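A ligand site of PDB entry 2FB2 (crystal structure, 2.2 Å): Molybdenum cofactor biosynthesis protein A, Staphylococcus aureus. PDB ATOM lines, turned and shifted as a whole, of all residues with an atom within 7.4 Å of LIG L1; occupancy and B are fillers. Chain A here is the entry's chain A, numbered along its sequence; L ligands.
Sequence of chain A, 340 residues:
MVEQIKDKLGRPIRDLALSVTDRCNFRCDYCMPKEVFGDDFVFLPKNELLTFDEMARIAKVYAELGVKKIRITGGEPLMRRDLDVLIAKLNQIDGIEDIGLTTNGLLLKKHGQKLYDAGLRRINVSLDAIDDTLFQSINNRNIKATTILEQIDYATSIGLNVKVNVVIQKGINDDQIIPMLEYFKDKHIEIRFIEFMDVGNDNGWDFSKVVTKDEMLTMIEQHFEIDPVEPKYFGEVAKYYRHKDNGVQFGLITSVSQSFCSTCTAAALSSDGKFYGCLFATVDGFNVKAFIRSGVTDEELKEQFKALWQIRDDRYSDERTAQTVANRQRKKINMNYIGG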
ATOM      1  N   ASP A  22      25.203  -4.686  -8.413  1.00  0.00           N
ATOM      2  CA  ASP A  22      25.366  -3.588  -9.339  1.00  0.00           C
ATOM      3  C   ASP A  22      24.037  -2.905  -9.709  1.00  0.00           C
ATOM      4  O   ASP A  22      24.014  -1.908 -10.450  1.00  0.00           O
ATOM      5  CB  ASP A  22      26.094  -4.071 -10.601  1.00  0.00           C
ATOM      6  CG  ASP A  22      25.364  -5.194 -11.320  1.00  0.00           C
ATOM      7  OD1 ASP A  22      24.615  -5.957 -10.670  1.00  0.00           O
ATOM      8  OD2 ASP A  22      25.558  -5.340 -12.560  1.00  0.00           O
ATOM      9  N   ARG A  23      22.934  -3.463  -9.240  1.00  0.00           N
ATOM     10  CA  ARG A  23      21.599  -2.981  -9.624  1.00  0.00           C
ATOM     11  C   ARG A  23      21.220  -1.813  -8.746  1.00  0.00           C
ATOM     12  O   ARG A  23      21.725  -1.678  -7.619  1.00  0.00           O
ATOM     13  CB  ARG A  23      20.573  -4.109  -9.398  1.00  0.00           C
ATOM     14  CG  ARG A  23      20.251  -4.946 -10.620  1.00  0.00           C
ATOM     15  CD  ARG A  23      21.232  -6.057 -10.763  1.00  0.00           C
ATOM     16  NE  ARG A  23      20.858  -7.009 -11.798  1.00  0.00           N
ATOM     17  CZ  ARG A  23      21.665  -7.983 -12.216  1.00  0.00           C
ATOM     18  NH1 ARG A  23      22.889  -8.118 -11.686  1.00  0.00           N
ATOM     19  NH2 ARG A  23      21.248  -8.832 -13.134  1.00  0.00           N
ATOM     20  N   CYS A  24      20.343  -0.948  -9.234  1.00  0.00           N
ATOM     21  CA  CYS A  24      19.818   0.117  -8.372  1.00  0.00           C
ATOM     22  C   CYS A  24      18.394   0.495  -8.727  1.00  0.00           C
ATOM     23  O   CYS A  24      17.945   0.312  -9.864  1.00  0.00           O
ATOM     24  CB  CYS A  24      20.752   1.334  -8.401  1.00  0.00           C
ATOM     25  SG  CYS A  24      20.329   2.675  -7.258  1.00  0.00           S
ATOM     26  N   ASN A  25      17.671   1.025  -7.738  1.00  0.00           N
ATOM     27  CA  ASN A  25      16.310   1.536  -8.029  1.00  0.00           C
ATOM     28  C   ASN A  25      16.248   3.024  -8.321  1.00  0.00           C
ATOM     29  O   ASN A  25      15.174   3.548  -8.657  1.00  0.00           O
ATOM     30  CB  ASN A  25      15.304   1.097  -6.967  1.00  0.00           C
ATOM     31  CG  ASN A  25      15.818   1.306  -5.499  1.00  0.00           C
ATOM     32  OD1 ASN A  25      16.804   1.983  -5.253  1.00  0.00           O
ATOM     33  ND2 ASN A  25      15.130   0.719  -4.555  1.00  0.00           N
ATOM     34  N   PHE A  26      17.376   3.728  -8.196  1.00  0.00           N
ATOM     35  CA  PHE A  26      17.468   5.124  -8.663  1.00  0.00           C
ATOM     36  C   PHE A  26      18.365   5.189  -9.908  1.00  0.00           C
ATOM     37  O   PHE A  26      19.081   4.223 -10.215  1.00  0.00           O
ATOM     38  CB  PHE A  26      18.090   6.012  -7.592  1.00  0.00           C
ATOM     39  CG  PHE A  26      17.212   6.282  -6.404  1.00  0.00           C
ATOM     40  CD1 PHE A  26      17.632   7.201  -5.437  1.00  0.00           C
ATOM     41  CD2 PHE A  26      15.982   5.619  -6.231  1.00  0.00           C
ATOM     42  CE1 PHE A  26      16.849   7.483  -4.324  1.00  0.00           C
ATOM     43  CE2 PHE A  26      15.202   5.866  -5.106  1.00  0.00           C
ATOM     44  CZ  PHE A  26      15.636   6.810  -4.139  1.00  0.00           C
ATOM     45  N   ARG A  27      18.325   6.334 -10.618  1.00  0.00           N
ATOM     46  CA  ARG A  27      19.291   6.656 -11.683  1.00  0.00           C
ATOM     47  C   ARG A  27      19.852   8.075 -11.464  1.00  0.00           C
ATOM     48  O   ARG A  27      19.691   8.992 -12.317  1.00  0.00           O
ATOM     49  CB  ARG A  27      18.676   6.545 -13.092  1.00  0.00           C
ATOM     50  CG  ARG A  27      18.386   5.108 -13.565  1.00  0.00           C
ATOM     51  CD  ARG A  27      19.640   4.188 -13.608  1.00  0.00           C
ATOM     52  NE  ARG A  27      19.332   2.887 -14.184  1.00  0.00           N
ATOM     53  CZ  ARG A  27      19.047   1.809 -13.472  1.00  0.00           C
ATOM     54  NH1 ARG A  27      19.097   1.851 -12.138  1.00  0.00           N
ATOM     55  NH2 ARG A  27      18.756   0.696 -14.085  1.00  0.00           N
ATOM     56  N   CYS A  28      20.481   8.259 -10.304  1.00  0.00           N
ATOM     57  CA  CYS A  28      21.069   9.550  -9.940  1.00  0.00           C
ATOM     58  C   CYS A  28      22.032  10.015 -11.046  1.00  0.00           C
ATOM     59  O   CYS A  28      22.863   9.240 -11.500  1.00  0.00           O
ATOM     60  CB  CYS A  28      21.775   9.478  -8.598  1.00  0.00           C
ATOM     61  SG  CYS A  28      20.736   8.716  -7.287  1.00  0.00           S
ATOM     62  N   ASP A  29      21.880  11.265 -11.461  1.00  0.00           N
ATOM     63  CA  ASP A  29      22.586  11.784 -12.646  1.00  0.00           C
ATOM     64  C   ASP A  29      24.099  11.615 -12.512  1.00  0.00           C
ATOM     65  O   ASP A  29      24.793  11.216 -13.458  1.00  0.00           O
ATOM     66  CB  ASP A  29      22.209  13.242 -12.898  1.00  0.00           C
ATOM     67  CG  ASP A  29      20.870  13.393 -13.622  1.00  0.00           C
ATOM     68  OD1 ASP A  29      19.947  14.079 -13.091  1.00  0.00           O
ATOM     69  OD2 ASP A  29      20.733  12.847 -14.752  1.00  0.00           O
ATOM     70  N   TYR A  30      24.609  11.868 -11.315  1.00  0.00           N
ATOM     71  CA  TYR A  30      26.044  11.907 -11.113  1.00  0.00           C
ATOM     72  C   TYR A  30      26.651  10.542 -10.791  1.00  0.00           C
ATOM     73  O   TYR A  30      27.860  10.443 -10.618  1.00  0.00           O
ATOM     74  CB  TYR A  30      26.397  12.952 -10.048  1.00  0.00           C
ATOM     75  CG  TYR A  30      25.914  12.648  -8.641  1.00  0.00           C
ATOM     76  CD1 TYR A  30      26.706  11.927  -7.760  1.00  0.00           C
ATOM     77  CD2 TYR A  30      24.671  13.130  -8.163  1.00  0.00           C
ATOM     78  CE1 TYR A  30      26.298  11.638  -6.451  1.00  0.00           C
ATOM     79  CE2 TYR A  30      24.240  12.847  -6.856  1.00  0.00           C
ATOM     80  CZ  TYR A  30      25.064  12.100  -6.004  1.00  0.00           C
ATOM     81  OH  TYR A  30      24.697  11.805  -4.712  1.00  0.00           O
ATOM     82  N   CYS A  31      25.820   9.494 -10.747  1.00  0.00           N
ATOM     83  CA  CYS A  31      26.251   8.146 -10.336  1.00  0.00           C
ATOM     84  C   CYS A  31      25.828   7.066 -11.340  1.00  0.00           C
ATOM     85  O   CYS A  31      26.678   6.367 -11.914  1.00  0.00           O
ATOM     86  CB  CYS A  31      25.668   7.820  -8.963  1.00  0.00           C
ATOM     87  SG  CYS A  31      26.059   6.139  -8.411  1.00  0.00           S
ATOM     88  N   MET A  32      24.506   6.937 -11.551  1.00  0.00           N
ATOM     89  CA  MET A  32      24.002   5.994 -12.536  1.00  0.00           C
ATOM     90  C   MET A  32      23.118   6.724 -13.545  1.00  0.00           C
ATOM     91  O   MET A  32      21.902   6.526 -13.570  1.00  0.00           O
ATOM     92  CB  MET A  32      23.282   4.811 -11.867  1.00  0.00           C
ATOM     93  CG  MET A  32      24.221   3.924 -11.068  1.00  0.00           C
ATOM     94  SD  MET A  32      23.448   2.497 -10.243  1.00  0.00           S
ATOM     95  CE  MET A  32      22.853   1.514 -11.631  1.00  0.00           C
ATOM     96  N   PRO A  33      23.730   7.573 -14.387  1.00  0.00           N
ATOM     97  CA  PRO A  33      22.874   8.373 -15.258  1.00  0.00           C
ATOM     98  C   PRO A  33      22.153   7.442 -16.229  1.00  0.00           C
ATOM     99  O   PRO A  33      22.727   6.457 -16.675  1.00  0.00           O
ATOM    100  CB  PRO A  33      23.871   9.298 -16.003  1.00  0.00           C
ATOM    101  CG  PRO A  33      25.182   8.611 -15.933  1.00  0.00           C
ATOM    102  CD  PRO A  33      25.171   7.828 -14.615  1.00  0.00           C
ATOM    103  N   THR A  73      27.356  -2.011   0.544  1.00  0.00           N
ATOM    104  CA  THR A  73      27.033  -0.987  -0.421  1.00  0.00           C
ATOM    105  C   THR A  73      26.684  -1.640  -1.762  1.00  0.00           C
ATOM    106  O   THR A  73      26.447  -2.859  -1.843  1.00  0.00           O
ATOM    107  CB  THR A  73      28.164   0.083  -0.491  1.00  0.00           C
ATOM    108  OG1 THR A  73      27.755   1.170  -1.344  1.00  0.00           O
ATOM    109  CG2 THR A  73      29.484  -0.524  -1.027  1.00  0.00           C
ATOM    110  N   GLY A  74      26.660  -0.837  -2.834  1.00  0.00           N
ATOM    111  CA  GLY A  74      26.220  -1.307  -4.142  1.00  0.00           C
ATOM    112  C   GLY A  74      26.656  -0.283  -5.184  1.00  0.00           C
ATOM    113  O   GLY A  74      27.714   0.314  -5.005  1.00  0.00           O
ATOM    114  N   GLY A  75      25.823   0.016  -6.185  1.00  0.00           N
ATOM    115  CA  GLY A  75      24.436  -0.425  -6.240  1.00  0.00           C
ATOM    116  C   GLY A  75      23.600   0.034  -5.043  1.00  0.00           C
ATOM    117  O   GLY A  75      24.090   0.717  -4.126  1.00  0.00           O
ATOM    118  N   GLU A  76      22.342  -0.353  -5.044  1.00  0.00           N
ATOM    119  CA  GLU A  76      21.509  -0.183  -3.885  1.00  0.00           C
ATOM    120  C   GLU A  76      21.460  -1.561  -3.211  1.00  0.00           C
ATOM    121  O   GLU A  76      20.851  -2.482  -3.739  1.00  0.00           O
ATOM    122  CB  GLU A  76      20.106   0.291  -4.290  1.00  0.00           C
ATOM    123  CG  GLU A  76      19.078   0.111  -3.212  1.00  0.00           C
ATOM    124  CD  GLU A  76      19.546   0.736  -1.865  1.00  0.00           C
ATOM    125  OE1 GLU A  76      19.247   0.123  -0.839  1.00  0.00           O
ATOM    126  OE2 GLU A  76      20.176   1.817  -1.851  1.00  0.00           O
ATOM    127  N   PRO A  77      22.108  -1.683  -2.056  1.00  0.00           N
ATOM    128  CA  PRO A  77      22.204  -3.006  -1.420  1.00  0.00           C
ATOM    129  C   PRO A  77      20.880  -3.710  -1.050  1.00  0.00           C
ATOM    130  O   PRO A  77      20.815  -4.941  -1.075  1.00  0.00           O
ATOM    131  CB  PRO A  77      23.065  -2.755  -0.175  1.00  0.00           C
ATOM    132  CG  PRO A  77      22.945  -1.243   0.083  1.00  0.00           C
ATOM    133  CD  PRO A  77      22.776  -0.616  -1.274  1.00  0.00           C
ATOM    134  N   THR A 102      25.037   1.394   3.569  1.00  0.00           N
ATOM    135  CA  THR A 102      24.786   2.638   2.872  1.00  0.00           C
ATOM    136  C   THR A 102      23.647   2.377   1.899  1.00  0.00           C
ATOM    137  O   THR A 102      23.754   1.514   1.051  1.00  0.00           O
ATOM    138  CB  THR A 102      26.047   3.088   2.113  1.00  0.00           C
ATOM    139  OG1 THR A 102      27.153   2.921   2.994  1.00  0.00           O
ATOM    140  CG2 THR A 102      25.971   4.538   1.730  1.00  0.00           C
ATOM    141  N   THR A 103      22.557   3.117   2.013  1.00  0.00           N
ATOM    142  CA  THR A 103      21.370   2.862   1.222  1.00  0.00           C
ATOM    143  C   THR A 103      20.692   4.188   0.873  1.00  0.00           C
ATOM    144  O   THR A 103      20.862   5.204   1.604  1.00  0.00           O
ATOM    145  CB  THR A 103      20.410   1.923   2.004  1.00  0.00           C
ATOM    146  OG1 THR A 103      19.228   1.656   1.253  1.00  0.00           O
ATOM    147  CG2 THR A 103      20.001   2.513   3.320  1.00  0.00           C
ATOM    148  N   ASN A 104      19.940   4.197  -0.239  1.00  0.00           N
ATOM    149  CA  ASN A 104      19.022   5.309  -0.521  1.00  0.00           C
ATOM    150  C   ASN A 104      17.783   5.218   0.371  1.00  0.00           C
ATOM    151  O   ASN A 104      16.961   6.132   0.399  1.00  0.00           O
ATOM    152  CB  ASN A 104      18.654   5.434  -2.026  1.00  0.00           C
ATOM    153  CG  ASN A 104      17.907   4.201  -2.581  1.00  0.00           C
ATOM    154  OD1 ASN A 104      17.107   3.581  -1.877  1.00  0.00           O
ATOM    155  ND2 ASN A 104      18.171   3.867  -3.858  1.00  0.00           N
ATOM    156  N   SER A 126      21.593   7.897   2.149  1.00  0.00           N
ATOM    157  CA  SER A 126      21.903   8.952   1.193  1.00  0.00           C
ATOM    158  C   SER A 126      20.627   9.672   0.747  1.00  0.00           C
ATOM    159  O   SER A 126      19.733   9.058   0.167  1.00  0.00           O
ATOM    160  CB  SER A 126      22.603   8.378  -0.038  1.00  0.00           C
ATOM    161  OG  SER A 126      23.754   7.659   0.354  1.00  0.00           O
ATOM    162  N   ASP A 128      19.695  13.497  -1.062  1.00  0.00           N
ATOM    163  CA  ASP A 128      20.323  14.681  -1.632  1.00  0.00           C
ATOM    164  C   ASP A 128      19.429  15.917  -1.653  1.00  0.00           C
ATOM    165  O   ASP A 128      19.874  16.981  -2.045  1.00  0.00           O
ATOM    166  CB  ASP A 128      20.906  14.394  -3.035  1.00  0.00           C
ATOM    167  CG  ASP A 128      22.313  13.774  -2.972  1.00  0.00           C
ATOM    168  OD1 ASP A 128      22.837  13.497  -1.854  1.00  0.00           O
ATOM    169  OD2 ASP A 128      22.897  13.558  -4.063  1.00  0.00           O
ATOM    170  N   ILE A 138      16.761  14.584  -9.368  1.00  0.00           N
ATOM    171  CA  ILE A 138      18.069  14.013  -9.062  1.00  0.00           C
ATOM    172  C   ILE A 138      18.074  12.475  -9.220  1.00  0.00           C
ATOM    173  O   ILE A 138      18.960  11.920  -9.848  1.00  0.00           O
ATOM    174  CB  ILE A 138      18.547  14.350  -7.615  1.00  0.00           C
ATOM    175  CG1 ILE A 138      18.790  15.867  -7.453  1.00  0.00           C
ATOM    176  CG2 ILE A 138      19.831  13.563  -7.254  1.00  0.00           C
ATOM    177  CD1 ILE A 138      18.989  16.301  -6.002  1.00  0.00           C
ATOM    178  N   ASN A 139      17.082  11.807  -8.633  1.00  0.00           N
ATOM    179  CA  ASN A 139      17.038  10.344  -8.722  1.00  0.00           C
ATOM    180  C   ASN A 139      16.501   9.783 -10.050  1.00  0.00           C
ATOM    181  O   ASN A 139      16.803   8.643 -10.403  1.00  0.00           O
ATOM    182  CB  ASN A 139      16.381   9.705  -7.497  1.00  0.00           C
ATOM    183  CG  ASN A 139      14.897  10.020  -7.366  1.00  0.00           C
ATOM    184  OD1 ASN A 139      14.097   9.697  -8.247  1.00  0.00           O
ATOM    185  ND2 ASN A 139      14.517  10.598  -6.227  1.00  0.00           N
HETATM  186 FE1  LIG L   1      21.921   4.366  -6.972  1.00  0.00          FE
HETATM  187 FE2  LIG L   1      21.878   6.907  -6.720  1.00  0.00          FE
HETATM  188 FE3  LIG L   1      23.028   5.170  -4.776  1.00  0.00          FE
HETATM  189 FE4  LIG L   1      24.046   5.669  -7.147  1.00  0.00          FE
HETATM  190  S1  LIG L   1      23.691   7.023  -5.633  1.00  0.00           S
HETATM  191  S2  LIG L   1      23.876   3.786  -6.192  1.00  0.00           S
HETATM  192  S3  LIG L   1      22.347   5.846  -8.499  1.00  0.00           S
HETATM  193  S4  LIG L   1      21.010   5.528  -5.446  1.00  0.00           S
HETATM  194  N1  LG2 L   2      22.919   3.168  -3.512  1.00  0.00           N
HETATM  195  C1  LG2 L   2      23.388   3.406  -2.129  1.00  0.00           C
HETATM  196  C2  LG2 L   2      23.301   4.899  -1.855  1.00  0.00           C
HETATM  197  O1  LG2 L   2      23.076   5.692  -2.802  1.00  0.00           O
HETATM  198  O2  LG2 L   2      23.491   5.316  -0.721  1.00  0.00           O
HETATM  199  C3  LG2 L   2      24.843   2.948  -1.870  1.00  0.00           C
HETATM  200  C4  LG2 L   2      25.851   3.052  -3.026  1.00  0.00           C
HETATM  201  S1  LG2 L   2      26.128   4.691  -3.719  1.00  0.00           S
HETATM  202  C5  LG2 L   2      27.315   4.459  -5.074  1.00  0.00           C
HETATM  203  C6  LG2 L   2      27.237   5.302  -2.421  1.00  0.00           C
HETATM  204  C7  LG2 L   2      27.478   6.815  -2.347  1.00  0.00           C
HETATM  205  O3  LG2 L   2      28.310   7.248  -3.413  1.00  0.00           O
HETATM  206  C8  LG2 L   2      26.218   7.684  -2.380  1.00  0.00           C
HETATM  207  O4  LG2 L   2      25.958   8.261  -1.089  1.00  0.00           O
HETATM  208  C9  LG2 L   2      26.598   8.717  -3.421  1.00  0.00           C
HETATM  209  O5  LG2 L   2      26.140  10.016  -3.137  1.00  0.00           O
HETATM  210  C10 LG2 L   2      28.127   8.635  -3.479  1.00  0.00           C
HETATM  211  N2  LG2 L   2      28.697   9.300  -4.678  1.00  0.00           N
HETATM  212  C11 LG2 L   2      28.666   8.853  -5.974  1.00  0.00           C
HETATM  213  N3  LG2 L   2      29.268   9.789  -6.759  1.00  0.00           N
HETATM  214  C12 LG2 L   2      29.690  10.828  -5.993  1.00  0.00           C
HETATM  215  C13 LG2 L   2      30.363  12.033  -6.269  1.00  0.00           C
HETATM  216  N4  LG2 L   2      30.714  12.344  -7.519  1.00  0.00           N
HETATM  217  N5  LG2 L   2      30.654  12.903  -5.236  1.00  0.00           N
HETATM  218  C14 LG2 L   2      30.291  12.605  -3.935  1.00  0.00           C
HETATM  219  N6  LG2 L   2      29.637  11.405  -3.664  1.00  0.00           N
HETATM  220  C15 LG2 L   2      29.332  10.535  -4.671  1.00  0.00           C
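SG of Cys 24 sits close to N of Phe 26 (3.3 Å). O of Cys 24 is in hydrogen-bond range of NH1 of Arg 27 (3.0 Å). The backbone NH (N) of Asn 104 sits at hydrogen-bond distance from the side-chain carboxylate (OE2) of Glu 76 (2.9 Å). OD1 of Asn 25 is in hydrogen-bond range of ND2 of Asn 104, at 2.7 Å.
N of Cys 28 sits close to S3 of LIG L1, 3.5 Å away. SG of Cys 28 binds FE2 of LIG L1, 2.2 Å away. The side-chain sulfur of Cys 24 binds an iron atom (FE1) of LIG L1, 2.3 Å away. The side-chain sulfur of Cys 31 binds an iron atom (FE4) of LIG L1, at 2.4 Å. ND2 of Asn 104 sits close to S4 of LIG L1 (3.7 Å). O of Gly 75 sits close to N1 of LG2 L2 (2.8 Å). OE2 of Glu 76 sits close to N1 of LG2 L2, at 3.5 Å. O5 of LG2 L2 sits at hydrogen-bond distance from OH of Tyr 30 (2.8 Å). An oxygen (O2) of LG2 L2 sits at hydrogen-bond distance from the side-chain hydroxyl of Ser 126 (2.6 Å).
The backbone carbonyl oxygen (O) of Gly 75 sits close to a sulfur (S2) of LIG L1. Residues that only touch LIG L1: Met 32 (3.6 Å) and Phe 26 (3.7 Å). Seven residues have an atom within 4 Å of LIG L1: Cys 24, Phe 26, Cys 28, Cys 31, Met 32, Gly 75 and Asn 104. The nearest printed residue that does not touch LIG L1 is Arg 27 (4.5 Å).
An oxygen (O1) of LG2 L2 is bound to an iron atom (FE3) of LIG L1, at 2.0 Å.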
